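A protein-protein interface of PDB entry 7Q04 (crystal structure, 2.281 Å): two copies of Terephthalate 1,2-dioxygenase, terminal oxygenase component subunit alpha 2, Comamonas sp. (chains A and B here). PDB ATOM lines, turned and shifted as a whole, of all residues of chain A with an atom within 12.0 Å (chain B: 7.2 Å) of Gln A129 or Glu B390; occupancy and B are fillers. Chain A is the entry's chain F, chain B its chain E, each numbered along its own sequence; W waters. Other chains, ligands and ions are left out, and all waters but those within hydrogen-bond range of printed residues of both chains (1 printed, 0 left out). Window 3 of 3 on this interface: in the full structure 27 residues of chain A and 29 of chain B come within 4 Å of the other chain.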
ATOM      1  N   VAL A 120     -13.656 -16.946 -16.599  1.00  0.00           N
ATOM      2  CA  VAL A 120     -12.602 -16.171 -15.894  1.00  0.00           C
ATOM      3  C   VAL A 120     -12.534 -16.679 -14.468  1.00  0.00           C
ATOM      4  O   VAL A 120     -13.466 -16.476 -13.734  1.00  0.00           O
ATOM      5  CB  VAL A 120     -12.870 -14.656 -15.958  1.00  0.00           C
ATOM      6  CG1 VAL A 120     -11.932 -13.874 -15.055  1.00  0.00           C
ATOM      7  CG2 VAL A 120     -12.818 -14.142 -17.396  1.00  0.00           C
ATOM      8  N   ALA A 121     -11.431 -17.314 -14.101  1.00  0.00           N
ATOM      9  CA  ALA A 121     -11.246 -17.857 -12.729  1.00  0.00           C
ATOM     10  C   ALA A 121     -11.433 -16.702 -11.751  1.00  0.00           C
ATOM     11  O   ALA A 121     -10.860 -15.611 -12.008  1.00  0.00           O
ATOM     12  CB  ALA A 121      -9.900 -18.511 -12.560  1.00  0.00           C
ATOM     13  N   PHE A 122     -12.277 -16.931 -10.740  1.00  0.00           N
ATOM     14  CA  PHE A 122     -12.599 -15.991  -9.639  1.00  0.00           C
ATOM     15  C   PHE A 122     -13.136 -14.655 -10.191  1.00  0.00           C
ATOM     16  O   PHE A 122     -12.875 -13.589  -9.603  1.00  0.00           O
ATOM     17  CB  PHE A 122     -11.345 -15.737  -8.800  1.00  0.00           C
ATOM     18  CG  PHE A 122     -10.621 -16.955  -8.282  1.00  0.00           C
ATOM     19  CD1 PHE A 122     -11.279 -18.162  -8.068  1.00  0.00           C
ATOM     20  CD2 PHE A 122      -9.290 -16.855  -7.933  1.00  0.00           C
ATOM     21  CE1 PHE A 122     -10.602 -19.258  -7.554  1.00  0.00           C
ATOM     22  CE2 PHE A 122      -8.610 -17.956  -7.430  1.00  0.00           C
ATOM     23  CZ  PHE A 122      -9.273 -19.149  -7.227  1.00  0.00           C
ATOM     24  N   GLU A 123     -13.885 -14.679 -11.294  1.00  0.00           N
ATOM     25  CA  GLU A 123     -14.472 -13.444 -11.860  1.00  0.00           C
ATOM     26  C   GLU A 123     -15.328 -12.753 -10.783  1.00  0.00           C
ATOM     27  O   GLU A 123     -15.341 -11.480 -10.756  1.00  0.00           O
ATOM     28  CB  GLU A 123     -15.333 -13.761 -13.075  1.00  0.00           C
ATOM     29  CG  GLU A 123     -15.829 -12.519 -13.789  1.00  0.00           C
ATOM     30  CD  GLU A 123     -16.638 -12.809 -15.047  1.00  0.00           C
ATOM     31  OE1 GLU A 123     -16.584 -13.941 -15.581  1.00  0.00           O
ATOM     32  OE2 GLU A 123     -17.310 -11.894 -15.498  1.00  0.00           O
ATOM     33  N   LYS A 124     -15.989 -13.551  -9.929  1.00  0.00           N
ATOM     34  CA  LYS A 124     -16.952 -13.083  -8.896  1.00  0.00           C
ATOM     35  C   LYS A 124     -16.290 -13.106  -7.517  1.00  0.00           C
ATOM     36  O   LYS A 124     -17.026 -13.160  -6.521  1.00  0.00           O
ATOM     37  CB  LYS A 124     -18.224 -13.942  -8.936  1.00  0.00           C
ATOM     38  CG  LYS A 124     -19.125 -13.717 -10.157  1.00  0.00           C
ATOM     39  CD  LYS A 124     -19.837 -12.332 -10.216  1.00  0.00           C
ATOM     40  CE  LYS A 124     -19.324 -11.298 -11.218  1.00  0.00           C
ATOM     41  NZ  LYS A 124     -19.790 -11.547 -12.602  1.00  0.00           N
ATOM     42  N   GLY A 125     -14.955 -13.035  -7.461  1.00  0.00           N
ATOM     43  CA  GLY A 125     -14.200 -13.039  -6.194  1.00  0.00           C
ATOM     44  C   GLY A 125     -14.181 -14.421  -5.555  1.00  0.00           C
ATOM     45  O   GLY A 125     -14.623 -15.396  -6.217  1.00  0.00           O
ATOM     46  N   VAL A 126     -13.637 -14.499  -4.336  1.00  0.00           N
ATOM     47  CA  VAL A 126     -13.621 -15.679  -3.411  1.00  0.00           C
ATOM     48  C   VAL A 126     -14.140 -15.200  -2.057  1.00  0.00           C
ATOM     49  O   VAL A 126     -13.442 -14.352  -1.457  1.00  0.00           O
ATOM     50  CB  VAL A 126     -12.190 -16.238  -3.251  1.00  0.00           C
ATOM     51  CG1 VAL A 126     -12.146 -17.507  -2.403  1.00  0.00           C
ATOM     52  CG2 VAL A 126     -11.517 -16.476  -4.590  1.00  0.00           C
ATOM     53  N   LYS A 127     -15.305 -15.694  -1.622  1.00  0.00           N
ATOM     54  CA  LYS A 127     -16.030 -15.259  -0.384  1.00  0.00           C
ATOM     55  C   LYS A 127     -16.306 -13.745  -0.440  1.00  0.00           C
ATOM     56  O   LYS A 127     -15.861 -13.000   0.482  1.00  0.00           O
ATOM     57  CB  LYS A 127     -15.245 -15.631   0.877  1.00  0.00           C
ATOM     58  CG  LYS A 127     -15.225 -17.119   1.202  1.00  0.00           C
ATOM     59  CD  LYS A 127     -14.085 -17.863   0.565  1.00  0.00           C
ATOM     60  CE  LYS A 127     -14.067 -19.323   0.961  1.00  0.00           C
ATOM     61  NZ  LYS A 127     -13.155 -19.554   2.109  1.00  0.00           N
ATOM     62  N   GLY A 128     -16.980 -13.311  -1.511  1.00  0.00           N
ATOM     63  CA  GLY A 128     -17.390 -11.912  -1.761  1.00  0.00           C
ATOM     64  C   GLY A 128     -16.238 -10.930  -1.664  1.00  0.00           C
ATOM     65  O   GLY A 128     -16.503  -9.755  -1.429  1.00  0.00           O
ATOM     66  N   GLN A 129     -15.003 -11.394  -1.862  1.00  0.00           N
ATOM     67  CA  GLN A 129     -13.775 -10.565  -1.823  1.00  0.00           C
ATOM     68  C   GLN A 129     -13.110 -10.564  -3.196  1.00  0.00           C
ATOM     69  O   GLN A 129     -12.923 -11.651  -3.772  1.00  0.00           O
ATOM     70  CB  GLN A 129     -12.822 -11.061  -0.735  1.00  0.00           C
ATOM     71  CG  GLN A 129     -12.940 -10.264   0.560  1.00  0.00           C
ATOM     72  CD  GLN A 129     -12.362 -11.032   1.716  1.00  0.00           C
ATOM     73  OE1 GLN A 129     -11.654 -12.031   1.549  1.00  0.00           O
ATOM     74  NE2 GLN A 129     -12.659 -10.543   2.902  1.00  0.00           N
ATOM     75  N   GLY A 130     -12.739  -9.368  -3.656  1.00  0.00           N
ATOM     76  CA  GLY A 130     -12.100  -9.108  -4.962  1.00  0.00           C
ATOM     77  C   GLY A 130     -12.887  -9.674  -6.135  1.00  0.00           C
ATOM     78  O   GLY A 130     -14.100  -9.723  -6.045  1.00  0.00           O
ATOM     79  N   GLY A 131     -12.202 -10.143  -7.184  1.00  0.00           N
ATOM     80  CA  GLY A 131     -12.834 -10.482  -8.465  1.00  0.00           C
ATOM     81  C   GLY A 131     -12.929  -9.246  -9.347  1.00  0.00           C
ATOM     82  O   GLY A 131     -12.309  -8.204  -9.012  1.00  0.00           O
ATOM     83  N   MET A 132     -13.689  -9.347 -10.439  1.00  0.00           N
ATOM     84  CA  MET A 132     -13.751  -8.292 -11.474  1.00  0.00           C
ATOM     85  C   MET A 132     -14.712  -7.206 -11.027  1.00  0.00           C
ATOM     86  O   MET A 132     -15.619  -7.477 -10.241  1.00  0.00           O
ATOM     87  CB  MET A 132     -14.184  -8.898 -12.813  1.00  0.00           C
ATOM     88  CG  MET A 132     -13.061  -9.789 -13.425  1.00  0.00           C
ATOM     89  SD  MET A 132     -11.528  -8.831 -13.668  1.00  0.00           S
ATOM     90  CE  MET A 132     -10.689  -9.955 -14.784  1.00  0.00           C
ATOM     91  N   PRO A 133     -14.536  -5.948 -11.495  1.00  0.00           N
ATOM     92  CA  PRO A 133     -15.516  -4.897 -11.230  1.00  0.00           C
ATOM     93  C   PRO A 133     -16.823  -5.254 -11.965  1.00  0.00           C
ATOM     94  O   PRO A 133     -16.782  -6.032 -12.920  1.00  0.00           O
ATOM     95  CB  PRO A 133     -14.845  -3.612 -11.742  1.00  0.00           C
ATOM     96  CG  PRO A 133     -13.878  -4.094 -12.819  1.00  0.00           C
ATOM     97  CD  PRO A 133     -13.451  -5.478 -12.369  1.00  0.00           C
ATOM     98  N   ALA A 134     -17.943  -4.706 -11.494  1.00  0.00           N
ATOM     99  CA  ALA A 134     -19.287  -4.938 -12.078  1.00  0.00           C
ATOM    100  C   ALA A 134     -19.244  -4.662 -13.587  1.00  0.00           C
ATOM    101  O   ALA A 134     -19.864  -5.445 -14.351  1.00  0.00           O
ATOM    102  CB  ALA A 134     -20.306  -4.079 -11.358  1.00  0.00           C
ATOM    103  N   LYS B 231      -7.459 -17.856   5.680  1.00  0.00           N
ATOM    104  CA  LYS B 231      -7.734 -16.525   5.079  1.00  0.00           C
ATOM    105  C   LYS B 231      -6.384 -16.001   4.582  1.00  0.00           C
ATOM    106  O   LYS B 231      -5.343 -16.394   5.102  1.00  0.00           O
ATOM    107  CB  LYS B 231      -8.373 -15.560   6.089  1.00  0.00           C
ATOM    108  CG  LYS B 231      -9.799 -15.910   6.494  1.00  0.00           C
ATOM    109  CD  LYS B 231     -10.313 -15.199   7.758  1.00  0.00           C
ATOM    110  CE  LYS B 231     -10.437 -13.700   7.582  1.00  0.00           C
ATOM    111  NZ  LYS B 231     -11.730 -13.194   8.102  1.00  0.00           N
ATOM    112  N   GLY B 232      -6.401 -15.063   3.656  1.00  0.00           N
ATOM    113  CA  GLY B 232      -5.190 -14.406   3.160  1.00  0.00           C
ATOM    114  C   GLY B 232      -5.444 -12.958   2.851  1.00  0.00           C
ATOM    115  O   GLY B 232      -6.580 -12.437   3.073  1.00  0.00           O
ATOM    116  N   GLY B 233      -4.405 -12.314   2.353  1.00  0.00           N
ATOM    117  CA  GLY B 233      -4.417 -10.863   2.134  1.00  0.00           C
ATOM    118  C   GLY B 233      -3.197 -10.420   1.366  1.00  0.00           C
ATOM    119  O   GLY B 233      -2.294 -11.219   1.136  1.00  0.00           O
ATOM    120  N   VAL B 234      -3.219  -9.167   0.973  1.00  0.00           N
ATOM    121  CA  VAL B 234      -2.195  -8.526   0.119  1.00  0.00           C
ATOM    122  C   VAL B 234      -2.008  -7.143   0.706  1.00  0.00           C
ATOM    123  O   VAL B 234      -2.982  -6.364   0.730  1.00  0.00           O
ATOM    124  CB  VAL B 234      -2.628  -8.452  -1.357  1.00  0.00           C
ATOM    125  CG1 VAL B 234      -1.588  -7.739  -2.217  1.00  0.00           C
ATOM    126  CG2 VAL B 234      -2.940  -9.838  -1.899  1.00  0.00           C
ATOM    127  N   TYR B 246       0.124 -12.965   1.840  1.00  0.00           N
ATOM    128  CA  TYR B 246       0.192 -13.879   3.006  1.00  0.00           C
ATOM    129  C   TYR B 246      -1.028 -14.799   2.994  1.00  0.00           C
ATOM    130  O   TYR B 246      -2.101 -14.452   2.394  1.00  0.00           O
ATOM    131  CB  TYR B 246       0.318 -13.093   4.321  1.00  0.00           C
ATOM    132  CG  TYR B 246      -0.905 -12.322   4.752  1.00  0.00           C
ATOM    133  CD1 TYR B 246      -1.925 -12.918   5.477  1.00  0.00           C
ATOM    134  CD2 TYR B 246      -1.050 -10.994   4.406  1.00  0.00           C
ATOM    135  CE1 TYR B 246      -3.068 -12.214   5.841  1.00  0.00           C
ATOM    136  CE2 TYR B 246      -2.177 -10.267   4.758  1.00  0.00           C
ATOM    137  CZ  TYR B 246      -3.201 -10.878   5.478  1.00  0.00           C
ATOM    138  OH  TYR B 246      -4.344 -10.196   5.827  1.00  0.00           O
ATOM    139  N   GLY B 382      -9.914  -6.651  -8.505  1.00  0.00           N
ATOM    140  CA  GLY B 382      -9.915  -5.830  -7.277  1.00  0.00           C
ATOM    141  C   GLY B 382     -10.045  -4.341  -7.574  1.00  0.00           C
ATOM    142  O   GLY B 382      -9.796  -3.536  -6.649  1.00  0.00           O
ATOM    143  N   HIS B 385      -7.555  -0.037  -7.563  1.00  0.00           N
ATOM    144  CA  HIS B 385      -6.806   0.418  -6.362  1.00  0.00           C
ATOM    145  C   HIS B 385      -5.421  -0.282  -6.374  1.00  0.00           C
ATOM    146  O   HIS B 385      -5.170  -1.264  -7.153  1.00  0.00           O
ATOM    147  CB  HIS B 385      -7.721   0.463  -5.103  1.00  0.00           C
ATOM    148  CG  HIS B 385      -7.568  -0.680  -4.161  1.00  0.00           C
ATOM    149  ND1 HIS B 385      -7.679  -1.994  -4.614  1.00  0.00           N
ATOM    150  CD2 HIS B 385      -7.321  -0.710  -2.823  1.00  0.00           C
ATOM    151  CE1 HIS B 385      -7.477  -2.802  -3.598  1.00  0.00           C
ATOM    152  NE2 HIS B 385      -7.239  -2.029  -2.476  1.00  0.00           N
ATOM    153  N   SER B 388      -3.611  -2.015   0.062  1.00  0.00           N
ATOM    154  CA  SER B 388      -3.821  -3.337   0.701  1.00  0.00           C
ATOM    155  C   SER B 388      -5.277  -3.815   0.541  1.00  0.00           C
ATOM    156  O   SER B 388      -6.171  -2.961   0.369  1.00  0.00           O
ATOM    157  CB  SER B 388      -3.400  -3.251   2.137  1.00  0.00           C
ATOM    158  OG  SER B 388      -2.149  -2.601   2.228  1.00  0.00           O
ATOM    159  N   SER B 389      -5.506  -5.132   0.596  1.00  0.00           N
ATOM    160  CA  SER B 389      -6.833  -5.785   0.406  1.00  0.00           C
ATOM    161  C   SER B 389      -6.886  -7.077   1.204  1.00  0.00           C
ATOM    162  O   SER B 389      -5.888  -7.792   1.181  1.00  0.00           O
ATOM    163  CB  SER B 389      -7.103  -6.157  -1.032  1.00  0.00           C
ATOM    164  OG  SER B 389      -7.331  -5.022  -1.840  1.00  0.00           O
ATOM    165  N   GLU B 390      -8.046  -7.414   1.753  1.00  0.00           N
ATOM    166  CA  GLU B 390      -8.327  -8.765   2.290  1.00  0.00           C
ATOM    167  C   GLU B 390      -8.529  -9.689   1.085  1.00  0.00           C
ATOM    168  O   GLU B 390      -9.004  -9.210   0.060  1.00  0.00           O
ATOM    169  CB  GLU B 390      -9.524  -8.724   3.243  1.00  0.00           C
ATOM    170  CG  GLU B 390      -9.142  -8.853   4.725  1.00  0.00           C
ATOM    171  CD  GLU B 390     -10.318  -8.730   5.688  1.00  0.00           C
ATOM    172  OE1 GLU B 390     -11.172  -7.842   5.433  1.00  0.00           O
ATOM    173  OE2 GLU B 390     -10.374  -9.501   6.709  1.00  0.00           O
ATOM    174  N   GLY B 391      -8.126 -10.940   1.202  1.00  0.00           N
ATOM    175  CA  GLY B 391      -8.256 -11.928   0.118  1.00  0.00           C
ATOM    176  C   GLY B 391      -7.189 -11.690  -0.936  1.00  0.00           C
ATOM    177  O   GLY B 391      -6.442 -10.661  -0.856  1.00  0.00           O
ATOM    178  N   ARG B 392      -7.051 -12.634  -1.868  1.00  0.00           N
ATOM    179  CA  ARG B 392      -5.937 -12.645  -2.847  1.00  0.00           C
ATOM    180  C   ARG B 392      -6.438 -12.675  -4.293  1.00  0.00           C
ATOM    181  O   ARG B 392      -5.554 -12.572  -5.181  1.00  0.00           O
ATOM    182  CB  ARG B 392      -5.028 -13.824  -2.511  1.00  0.00           C
ATOM    183  CG  ARG B 392      -4.159 -13.527  -1.296  1.00  0.00           C
ATOM    184  CD  ARG B 392      -3.130 -14.607  -1.050  1.00  0.00           C
ATOM    185  NE  ARG B 392      -3.677 -15.941  -0.809  1.00  0.00           N
ATOM    186  CZ  ARG B 392      -2.956 -17.057  -0.889  1.00  0.00           C
ATOM    187  NH1 ARG B 392      -1.684 -16.992  -1.284  1.00  0.00           N
ATOM    188  NH2 ARG B 392      -3.518 -18.232  -0.632  1.00  0.00           N
ATOM    189  N   ALA B 393      -7.749 -12.824  -4.538  1.00  0.00           N
ATOM    190  CA  ALA B 393      -8.326 -12.718  -5.901  1.00  0.00           C
ATOM    191  C   ALA B 393      -8.377 -11.235  -6.335  1.00  0.00           C
ATOM    192  O   ALA B 393      -9.446 -10.676  -6.562  1.00  0.00           O
ATOM    193  CB  ALA B 393      -9.659 -13.402  -5.926  1.00  0.00           C
ATOM    194  N   THR B 394      -7.205 -10.611  -6.424  1.00  0.00           N
ATOM    195  CA  THR B 394      -6.969  -9.188  -6.786  1.00  0.00           C
ATOM    196  C   THR B 394      -5.630  -9.080  -7.535  1.00  0.00           C
ATOM    197  O   THR B 394      -4.820 -10.028  -7.432  1.00  0.00           O
ATOM    198  CB  THR B 394      -6.956  -8.308  -5.543  1.00  0.00           C
ATOM    199  OG1 THR B 394      -6.650  -6.958  -5.903  1.00  0.00           O
ATOM    200  CG2 THR B 394      -5.951  -8.791  -4.545  1.00  0.00           C
HETATM  201  O   HOH W   1     -10.099 -12.244  -2.881  1.00  0.00           O
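No position is printed for both chains.
Of the 6 pairs that touch across the chains among the printed residues, none has its exchanged pair printed and touching as well.
Water W1 lies within hydrogen-bond range of the backbone NH (N) of Ala B393 (2.9 Å), the backbone carbonyl oxygen (O) of Gln A129 (3.0 Å) and the backbone NH (N) of Arg B392 (3.2 Å).
Printed residues of chain B that touch a printed residue of chain A: Gly B382, Glu B390, Gly B391 and Ala B393.
Along chain B the printed residues that touch a printed residue of chain A span positions 382 to 393.
Hydrophobic or aromatic side chains of chain A that line the printed part of chain B: Val A126.
Among the printed residues, 6 pairs touch across the chains.
Among the printed residues, no Asp or Glu carboxylate lies within 4 Å of a Lys or Arg side-chain nitrogen of the other chain.
The backbone carbonyl oxygen of Gly B382 sits at hydrogen-bond distance from a ring nitrogen (ND1) of His B385 (3.3 Å).
The backbone NH (N) of Gly B391 sits at hydrogen-bond distance from the backbone carbonyl oxygen (O) of Gly B232, at 2.9 Å.
Gln A129 touches just these residues of chain B: Glu B390 and Gly B391.
Glu B390 touches just one residue of chain A: Gln A129 (3.6 Å).
No residue of chain A comes within 4 Å of Gly B232.
No residue of chain A comes within 4 Å of Gly B233.
No residue of chain A comes within 4 Å of Ser B388.
Printed residues of chain A within 4 Å of Gly B382: Gly A131 (2.9 Å).
Printed residues of chain B within 4 Å of Gly A131: Gly B382 (2.9 Å) and Ala B393 (2.9 Å).
Of the printed residues of chain A, Ala B393 touches Val A126, Gly A130 and Gly A131.
Of the printed residues of chain B, Val A126 touches Ala B393 (3.8 Å).
The nearest residue of chain B that does not touch Gln A129 is Ala B393 (4.3 Å).
The nearest residue of chain A that does not touch Glu B390 is Gly A130 (5.3 Å).
The nearest printed residue of chain A that does not touch Ala B393 is Phe A122 (4.01 Å).
Among the printed residues, pairs that only touch across the chains: Val A126 with Ala B393, Gln A129 with Glu B390, Gln A129 with Gly B391 and Gly A130 with Ala B393.
O of Ala B393 lies within hydrogen-bond range of N of Gly A131 (2.9 Å).
The backbone NH (N) of Gly B382 is in hydrogen-bond range of the backbone carbonyl oxygen (O) of Gly A131, 2.9 Å away.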
